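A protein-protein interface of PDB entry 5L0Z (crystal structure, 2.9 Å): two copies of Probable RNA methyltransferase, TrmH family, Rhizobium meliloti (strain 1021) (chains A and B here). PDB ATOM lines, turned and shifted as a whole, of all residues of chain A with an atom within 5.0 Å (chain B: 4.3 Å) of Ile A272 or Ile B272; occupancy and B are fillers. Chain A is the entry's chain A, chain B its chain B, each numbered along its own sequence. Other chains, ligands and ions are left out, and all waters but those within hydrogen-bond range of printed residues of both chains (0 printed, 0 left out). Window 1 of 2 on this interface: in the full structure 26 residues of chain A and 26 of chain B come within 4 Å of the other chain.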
ATOM      1  N   TYR A 220     -16.716 -23.985   0.552  1.00  0.00           N
ATOM      2  CA  TYR A 220     -16.146 -24.534  -0.685  1.00  0.00           C
ATOM      3  C   TYR A 220     -15.067 -23.630  -1.311  1.00  0.00           C
ATOM      4  O   TYR A 220     -14.216 -24.121  -2.053  1.00  0.00           O
ATOM      5  CB  TYR A 220     -17.245 -24.879  -1.715  1.00  0.00           C
ATOM      6  CG  TYR A 220     -17.844 -23.695  -2.463  1.00  0.00           C
ATOM      7  CD1 TYR A 220     -18.557 -22.676  -1.790  1.00  0.00           C
ATOM      8  CD2 TYR A 220     -17.735 -23.605  -3.835  1.00  0.00           C
ATOM      9  CE1 TYR A 220     -19.110 -21.608  -2.468  1.00  0.00           C
ATOM     10  CE2 TYR A 220     -18.289 -22.536  -4.512  1.00  0.00           C
ATOM     11  CZ  TYR A 220     -18.980 -21.547  -3.818  1.00  0.00           C
ATOM     12  OH  TYR A 220     -19.523 -20.503  -4.508  1.00  0.00           O
ATOM     13  N   ILE A 255     -21.809 -24.850   0.176  1.00  0.00           N
ATOM     14  CA  ILE A 255     -22.009 -23.547  -0.456  1.00  0.00           C
ATOM     15  C   ILE A 255     -22.914 -22.725   0.454  1.00  0.00           C
ATOM     16  O   ILE A 255     -24.010 -23.193   0.836  1.00  0.00           O
ATOM     17  CB  ILE A 255     -22.638 -23.712  -1.849  1.00  0.00           C
ATOM     18  CG1 ILE A 255     -21.683 -24.471  -2.763  1.00  0.00           C
ATOM     19  CG2 ILE A 255     -22.988 -22.374  -2.481  1.00  0.00           C
ATOM     20  CD1 ILE A 255     -22.422 -25.185  -3.861  1.00  0.00           C
ATOM     21  N   ILE A 268     -27.251 -27.536 -10.082  1.00  0.00           N
ATOM     22  CA  ILE A 268     -26.839 -26.169  -9.836  1.00  0.00           C
ATOM     23  C   ILE A 268     -25.629 -26.155  -8.941  1.00  0.00           C
ATOM     24  O   ILE A 268     -24.637 -25.524  -9.264  1.00  0.00           O
ATOM     25  CB  ILE A 268     -28.019 -25.331  -9.281  1.00  0.00           C
ATOM     26  CG1 ILE A 268     -29.030 -25.090 -10.398  1.00  0.00           C
ATOM     27  CG2 ILE A 268     -27.565 -23.994  -8.697  1.00  0.00           C
ATOM     28  CD1 ILE A 268     -28.611 -24.068 -11.450  1.00  0.00           C
ATOM     29  N   ALA A 269     -25.752 -26.874  -7.833  1.00  0.00           N
ATOM     30  CA  ALA A 269     -24.668 -27.137  -6.911  1.00  0.00           C
ATOM     31  C   ALA A 269     -23.453 -27.716  -7.639  1.00  0.00           C
ATOM     32  O   ALA A 269     -22.344 -27.255  -7.458  1.00  0.00           O
ATOM     33  CB  ALA A 269     -25.140 -28.099  -5.843  1.00  0.00           C
ATOM     34  N   THR A 270     -23.670 -28.691  -8.508  1.00  0.00           N
ATOM     35  CA  THR A 270     -22.556 -29.325  -9.184  1.00  0.00           C
ATOM     36  C   THR A 270     -21.803 -28.346 -10.107  1.00  0.00           C
ATOM     37  O   THR A 270     -20.555 -28.376 -10.185  1.00  0.00           O
ATOM     38  CB  THR A 270     -23.028 -30.566  -9.918  1.00  0.00           C
ATOM     39  OG1 THR A 270     -23.894 -31.316  -9.043  1.00  0.00           O
ATOM     40  CG2 THR A 270     -21.834 -31.411 -10.330  1.00  0.00           C
ATOM     41  N   GLY A 271     -22.550 -27.463 -10.749  1.00  0.00           N
ATOM     42  CA  GLY A 271     -22.001 -26.414 -11.567  1.00  0.00           C
ATOM     43  C   GLY A 271     -21.203 -25.438 -10.750  1.00  0.00           C
ATOM     44  O   GLY A 271     -20.089 -25.086 -11.141  1.00  0.00           O
ATOM     45  N   ILE A 272     -21.758 -25.020  -9.617  1.00  0.00           N
ATOM     46  CA  ILE A 272     -21.072 -24.086  -8.714  1.00  0.00           C
ATOM     47  C   ILE A 272     -19.673 -24.622  -8.296  1.00  0.00           C
ATOM     48  O   ILE A 272     -18.662 -23.898  -8.279  1.00  0.00           O
ATOM     49  CB  ILE A 272     -21.951 -23.810  -7.471  1.00  0.00           C
ATOM     50  CG1 ILE A 272     -23.152 -22.940  -7.831  1.00  0.00           C
ATOM     51  CG2 ILE A 272     -21.173 -23.132  -6.353  1.00  0.00           C
ATOM     52  CD1 ILE A 272     -22.832 -21.495  -8.151  1.00  0.00           C
ATOM     53  N   MET A 273     -19.662 -25.912  -7.989  1.00  0.00           N
ATOM     54  CA  MET A 273     -18.494 -26.612  -7.543  1.00  0.00           C
ATOM     55  C   MET A 273     -17.579 -26.865  -8.704  1.00  0.00           C
ATOM     56  O   MET A 273     -16.360 -26.751  -8.555  1.00  0.00           O
ATOM     57  CB  MET A 273     -18.901 -27.930  -6.890  1.00  0.00           C
ATOM     58  CG  MET A 273     -19.800 -27.755  -5.661  1.00  0.00           C
ATOM     59  SD  MET A 273     -18.869 -27.100  -4.057  1.00  0.00           S
ATOM     60  CE  MET A 273     -17.328 -28.310  -3.871  1.00  0.00           C
ATOM     61  N   LEU A 274     -18.109 -27.203  -9.871  1.00  0.00           N
ATOM     62  CA  LEU A 274     -17.202 -27.415 -10.980  1.00  0.00           C
ATOM     63  C   LEU A 274     -16.331 -26.206 -11.228  1.00  0.00           C
ATOM     64  O   LEU A 274     -15.148 -26.330 -11.439  1.00  0.00           O
ATOM     65  CB  LEU A 274     -17.944 -27.751 -12.237  1.00  0.00           C
ATOM     66  CG  LEU A 274     -18.220 -29.239 -12.296  1.00  0.00           C
ATOM     67  CD1 LEU A 274     -19.375 -29.495 -13.278  1.00  0.00           C
ATOM     68  CD2 LEU A 274     -16.960 -30.050 -12.668  1.00  0.00           C
ATOM     69  N   PHE A 275     -16.919 -25.030 -11.163  1.00  0.00           N
ATOM     70  CA  PHE A 275     -16.194 -23.797 -11.494  1.00  0.00           C
ATOM     71  C   PHE A 275     -15.433 -23.145 -10.346  1.00  0.00           C
ATOM     72  O   PHE A 275     -14.717 -22.177 -10.557  1.00  0.00           O
ATOM     73  CB  PHE A 275     -17.162 -22.789 -12.118  1.00  0.00           C
ATOM     74  CG  PHE A 275     -17.523 -23.134 -13.508  1.00  0.00           C
ATOM     75  CD1 PHE A 275     -18.382 -24.181 -13.761  1.00  0.00           C
ATOM     76  CD2 PHE A 275     -16.956 -22.459 -14.562  1.00  0.00           C
ATOM     77  CE1 PHE A 275     -18.695 -24.538 -15.052  1.00  0.00           C
ATOM     78  CE2 PHE A 275     -17.265 -22.794 -15.859  1.00  0.00           C
ATOM     79  CZ  PHE A 275     -18.131 -23.840 -16.108  1.00  0.00           C
ATOM     80  N   GLU A 276     -15.623 -23.640  -9.137  1.00  0.00           N
ATOM     81  CA  GLU A 276     -14.759 -23.287  -8.055  1.00  0.00           C
ATOM     82  C   GLU A 276     -13.548 -24.197  -8.075  1.00  0.00           C
ATOM     83  O   GLU A 276     -12.409 -23.746  -8.094  1.00  0.00           O
ATOM     84  CB  GLU A 276     -15.490 -23.460  -6.753  1.00  0.00           C
ATOM     85  CG  GLU A 276     -14.701 -22.854  -5.626  1.00  0.00           C
ATOM     86  CD  GLU A 276     -14.509 -21.375  -5.838  1.00  0.00           C
ATOM     87  OE1 GLU A 276     -15.423 -20.759  -6.445  1.00  0.00           O
ATOM     88  OE2 GLU A 276     -13.444 -20.867  -5.406  1.00  0.00           O
ATOM     89  N   TYR B 220     -15.874 -13.010 -16.035  1.00  0.00           N
ATOM     90  CA  TYR B 220     -16.873 -12.732 -15.035  1.00  0.00           C
ATOM     91  C   TYR B 220     -16.341 -12.585 -13.625  1.00  0.00           C
ATOM     92  O   TYR B 220     -16.992 -11.945 -12.788  1.00  0.00           O
ATOM     93  CB  TYR B 220     -17.954 -13.801 -15.083  1.00  0.00           C
ATOM     94  CG  TYR B 220     -17.635 -15.103 -14.387  1.00  0.00           C
ATOM     95  CD1 TYR B 220     -16.658 -15.985 -14.866  1.00  0.00           C
ATOM     96  CD2 TYR B 220     -18.333 -15.475 -13.237  1.00  0.00           C
ATOM     97  CE1 TYR B 220     -16.387 -17.178 -14.195  1.00  0.00           C
ATOM     98  CE2 TYR B 220     -18.048 -16.667 -12.574  1.00  0.00           C
ATOM     99  CZ  TYR B 220     -17.102 -17.510 -13.064  1.00  0.00           C
ATOM    100  OH  TYR B 220     -16.903 -18.656 -12.394  1.00  0.00           O
ATOM    101  N   ILE B 255     -18.394 -16.434 -18.856  1.00  0.00           N
ATOM    102  CA  ILE B 255     -17.837 -17.486 -18.046  1.00  0.00           C
ATOM    103  C   ILE B 255     -16.979 -18.355 -18.985  1.00  0.00           C
ATOM    104  O   ILE B 255     -17.502 -18.928 -19.935  1.00  0.00           O
ATOM    105  CB  ILE B 255     -18.970 -18.334 -17.428  1.00  0.00           C
ATOM    106  CG1 ILE B 255     -19.934 -17.461 -16.642  1.00  0.00           C
ATOM    107  CG2 ILE B 255     -18.418 -19.407 -16.505  1.00  0.00           C
ATOM    108  CD1 ILE B 255     -21.166 -18.190 -16.190  1.00  0.00           C
ATOM    109  N   ILE B 268     -27.745 -22.820 -15.152  1.00  0.00           N
ATOM    110  CA  ILE B 268     -26.398 -23.097 -14.671  1.00  0.00           C
ATOM    111  C   ILE B 268     -25.615 -21.803 -14.785  1.00  0.00           C
ATOM    112  O   ILE B 268     -25.110 -21.305 -13.779  1.00  0.00           O
ATOM    113  CB  ILE B 268     -25.729 -24.258 -15.454  1.00  0.00           C
ATOM    114  CG1 ILE B 268     -26.487 -25.582 -15.204  1.00  0.00           C
ATOM    115  CG2 ILE B 268     -24.253 -24.381 -15.115  1.00  0.00           C
ATOM    116  CD1 ILE B 268     -26.155 -26.335 -13.930  1.00  0.00           C
ATOM    117  N   ALA B 269     -25.542 -21.233 -15.974  1.00  0.00           N
ATOM    118  CA  ALA B 269     -24.870 -19.951 -16.112  1.00  0.00           C
ATOM    119  C   ALA B 269     -25.362 -18.980 -15.008  1.00  0.00           C
ATOM    120  O   ALA B 269     -24.521 -18.462 -14.255  1.00  0.00           O
ATOM    121  CB  ALA B 269     -25.065 -19.365 -17.495  1.00  0.00           C
ATOM    122  N   THR B 270     -26.688 -18.817 -14.836  1.00  0.00           N
ATOM    123  CA  THR B 270     -27.254 -17.860 -13.854  1.00  0.00           C
ATOM    124  C   THR B 270     -26.835 -18.185 -12.424  1.00  0.00           C
ATOM    125  O   THR B 270     -26.535 -17.302 -11.658  1.00  0.00           O
ATOM    126  CB  THR B 270     -28.811 -17.790 -13.888  1.00  0.00           C
ATOM    127  OG1 THR B 270     -29.291 -17.801 -15.230  1.00  0.00           O
ATOM    128  CG2 THR B 270     -29.342 -16.536 -13.169  1.00  0.00           C
ATOM    129  N   GLY B 271     -26.829 -19.449 -12.056  1.00  0.00           N
ATOM    130  CA  GLY B 271     -26.353 -19.813 -10.733  1.00  0.00           C
ATOM    131  C   GLY B 271     -24.901 -19.378 -10.500  1.00  0.00           C
ATOM    132  O   GLY B 271     -24.577 -18.662  -9.499  1.00  0.00           O
ATOM    133  N   ILE B 272     -24.025 -19.752 -11.444  1.00  0.00           N
ATOM    134  CA  ILE B 272     -22.622 -19.286 -11.386  1.00  0.00           C
ATOM    135  C   ILE B 272     -22.474 -17.765 -11.265  1.00  0.00           C
ATOM    136  O   ILE B 272     -21.660 -17.290 -10.496  1.00  0.00           O
ATOM    137  CB  ILE B 272     -21.815 -19.829 -12.569  1.00  0.00           C
ATOM    138  CG1 ILE B 272     -21.551 -21.303 -12.305  1.00  0.00           C
ATOM    139  CG2 ILE B 272     -20.481 -19.125 -12.731  1.00  0.00           C
ATOM    140  CD1 ILE B 272     -21.228 -22.104 -13.553  1.00  0.00           C
ATOM    141  N   MET B 273     -23.256 -17.020 -12.014  1.00  0.00           N
ATOM    142  CA  MET B 273     -23.148 -15.579 -11.963  1.00  0.00           C
ATOM    143  C   MET B 273     -23.608 -15.079 -10.614  1.00  0.00           C
ATOM    144  O   MET B 273     -22.960 -14.226  -9.999  1.00  0.00           O
ATOM    145  CB  MET B 273     -23.967 -14.928 -13.081  1.00  0.00           C
ATOM    146  CG  MET B 273     -23.470 -15.191 -14.479  1.00  0.00           C
ATOM    147  SD  MET B 273     -21.674 -14.410 -14.701  1.00  0.00           S
ATOM    148  CE  MET B 273     -21.931 -12.478 -14.472  1.00  0.00           C
ATOM    149  N   LEU B 274     -24.743 -15.592 -10.160  1.00  0.00           N
ATOM    150  CA  LEU B 274     -25.239 -15.271  -8.845  1.00  0.00           C
ATOM    151  C   LEU B 274     -24.198 -15.412  -7.759  1.00  0.00           C
ATOM    152  O   LEU B 274     -24.014 -14.521  -6.985  1.00  0.00           O
ATOM    153  CB  LEU B 274     -26.411 -16.147  -8.493  1.00  0.00           C
ATOM    154  CG  LEU B 274     -27.731 -15.499  -8.845  1.00  0.00           C
ATOM    155  CD1 LEU B 274     -28.810 -16.581  -8.826  1.00  0.00           C
ATOM    156  CD2 LEU B 274     -28.101 -14.386  -7.865  1.00  0.00           C
ATOM    157  N   PHE B 275     -23.501 -16.526  -7.710  1.00  0.00           N
ATOM    158  CA  PHE B 275     -22.532 -16.749  -6.614  1.00  0.00           C
ATOM    159  C   PHE B 275     -21.207 -15.994  -6.710  1.00  0.00           C
ATOM    160  O   PHE B 275     -20.483 -15.890  -5.719  1.00  0.00           O
ATOM    161  CB  PHE B 275     -22.326 -18.235  -6.393  1.00  0.00           C
ATOM    162  CG  PHE B 275     -23.424 -18.821  -5.627  1.00  0.00           C
ATOM    163  CD1 PHE B 275     -24.653 -18.984  -6.205  1.00  0.00           C
ATOM    164  CD2 PHE B 275     -23.279 -19.090  -4.315  1.00  0.00           C
ATOM    165  CE1 PHE B 275     -25.734 -19.473  -5.501  1.00  0.00           C
ATOM    166  CE2 PHE B 275     -24.344 -19.578  -3.579  1.00  0.00           C
ATOM    167  CZ  PHE B 275     -25.580 -19.776  -4.174  1.00  0.00           C
ATOM    168  N   GLU B 276     -20.911 -15.470  -7.892  1.00  0.00           N
ATOM    169  CA  GLU B 276     -19.775 -14.601  -8.080  1.00  0.00           C
ATOM    170  C   GLU B 276     -20.198 -13.216  -7.699  1.00  0.00           C
ATOM    171  O   GLU B 276     -19.495 -12.543  -6.958  1.00  0.00           O
ATOM    172  CB  GLU B 276     -19.299 -14.604  -9.539  1.00  0.00           C
ATOM    173  CG  GLU B 276     -17.819 -14.275  -9.733  1.00  0.00           C
ATOM    174  CD  GLU B 276     -16.918 -15.350  -9.152  1.00  0.00           C
ATOM    175  OE1 GLU B 276     -17.140 -16.547  -9.438  1.00  0.00           O
ATOM    176  OE2 GLU B 276     -15.984 -15.014  -8.401  1.00  0.00           O
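Phe B275 touches Ile A255.
Ile A272 touches Gly B271.
CD1 of Ile A272 touches N of Ile B272, 3.9 Å away.
Ile A272 touches Phe B275 (CD1 to CD1, 3.7 Å).
CE2 of Phe A275 touches CG2 of Ile B255, 3.6 Å away.
Phe A275 touches Ile B272 (CD1 to CD1, 3.5 Å).
Ile A255 touches Phe B275, and with the chains exchanged Phe A275 touches Ile B255.
Ile A272 touches Gly B271, but with the chains exchanged Gly A271 does not touch Ile B272 (4.001 Å).
Ile B272 touches its own counterpart, Ile A272.
Ile A272 touches Phe B275, and with the chains exchanged Phe A275 touches Ile B272.
11 positions are printed for both chains.
Of the 6 pairs that touch across the chains among the printed residues, 5 have their exchanged pair printed and touching as well.
Hydrophobic or aromatic side chains of chain A that line the printed part of chain B: Ile A255, Ile A272 and Phe A275.
Of the 11 printed residues of chain B, 4 touch a printed residue of chain A.
Hydrophobic or aromatic side chains of chain B that line the printed part of chain A: Ile B255, Ile B272 and Phe B275.
Of the printed residues of chain B, Ile A255 touches Phe B275.
Of the printed residues of chain B, Ile A272 touches Gly B271, Ile B272 and Phe B275.
Met A273 touches none of the printed residues of chain B.
Tyr B220 touches none of the printed residues of chain A.
Of the printed residues of chain A, Ile B255 touches Phe A275.
Printed residues of chain A within 4 Å of Ile B272: Ile A272 and Phe A275.
Printed residues of chain A within 4 Å of Phe B275: Ile A255 (3.3 Å) and Ile A272 (3.7 Å).
The nearest printed residue of chain A that does not touch Gly B271 is Ile A268 (4.8 Å).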
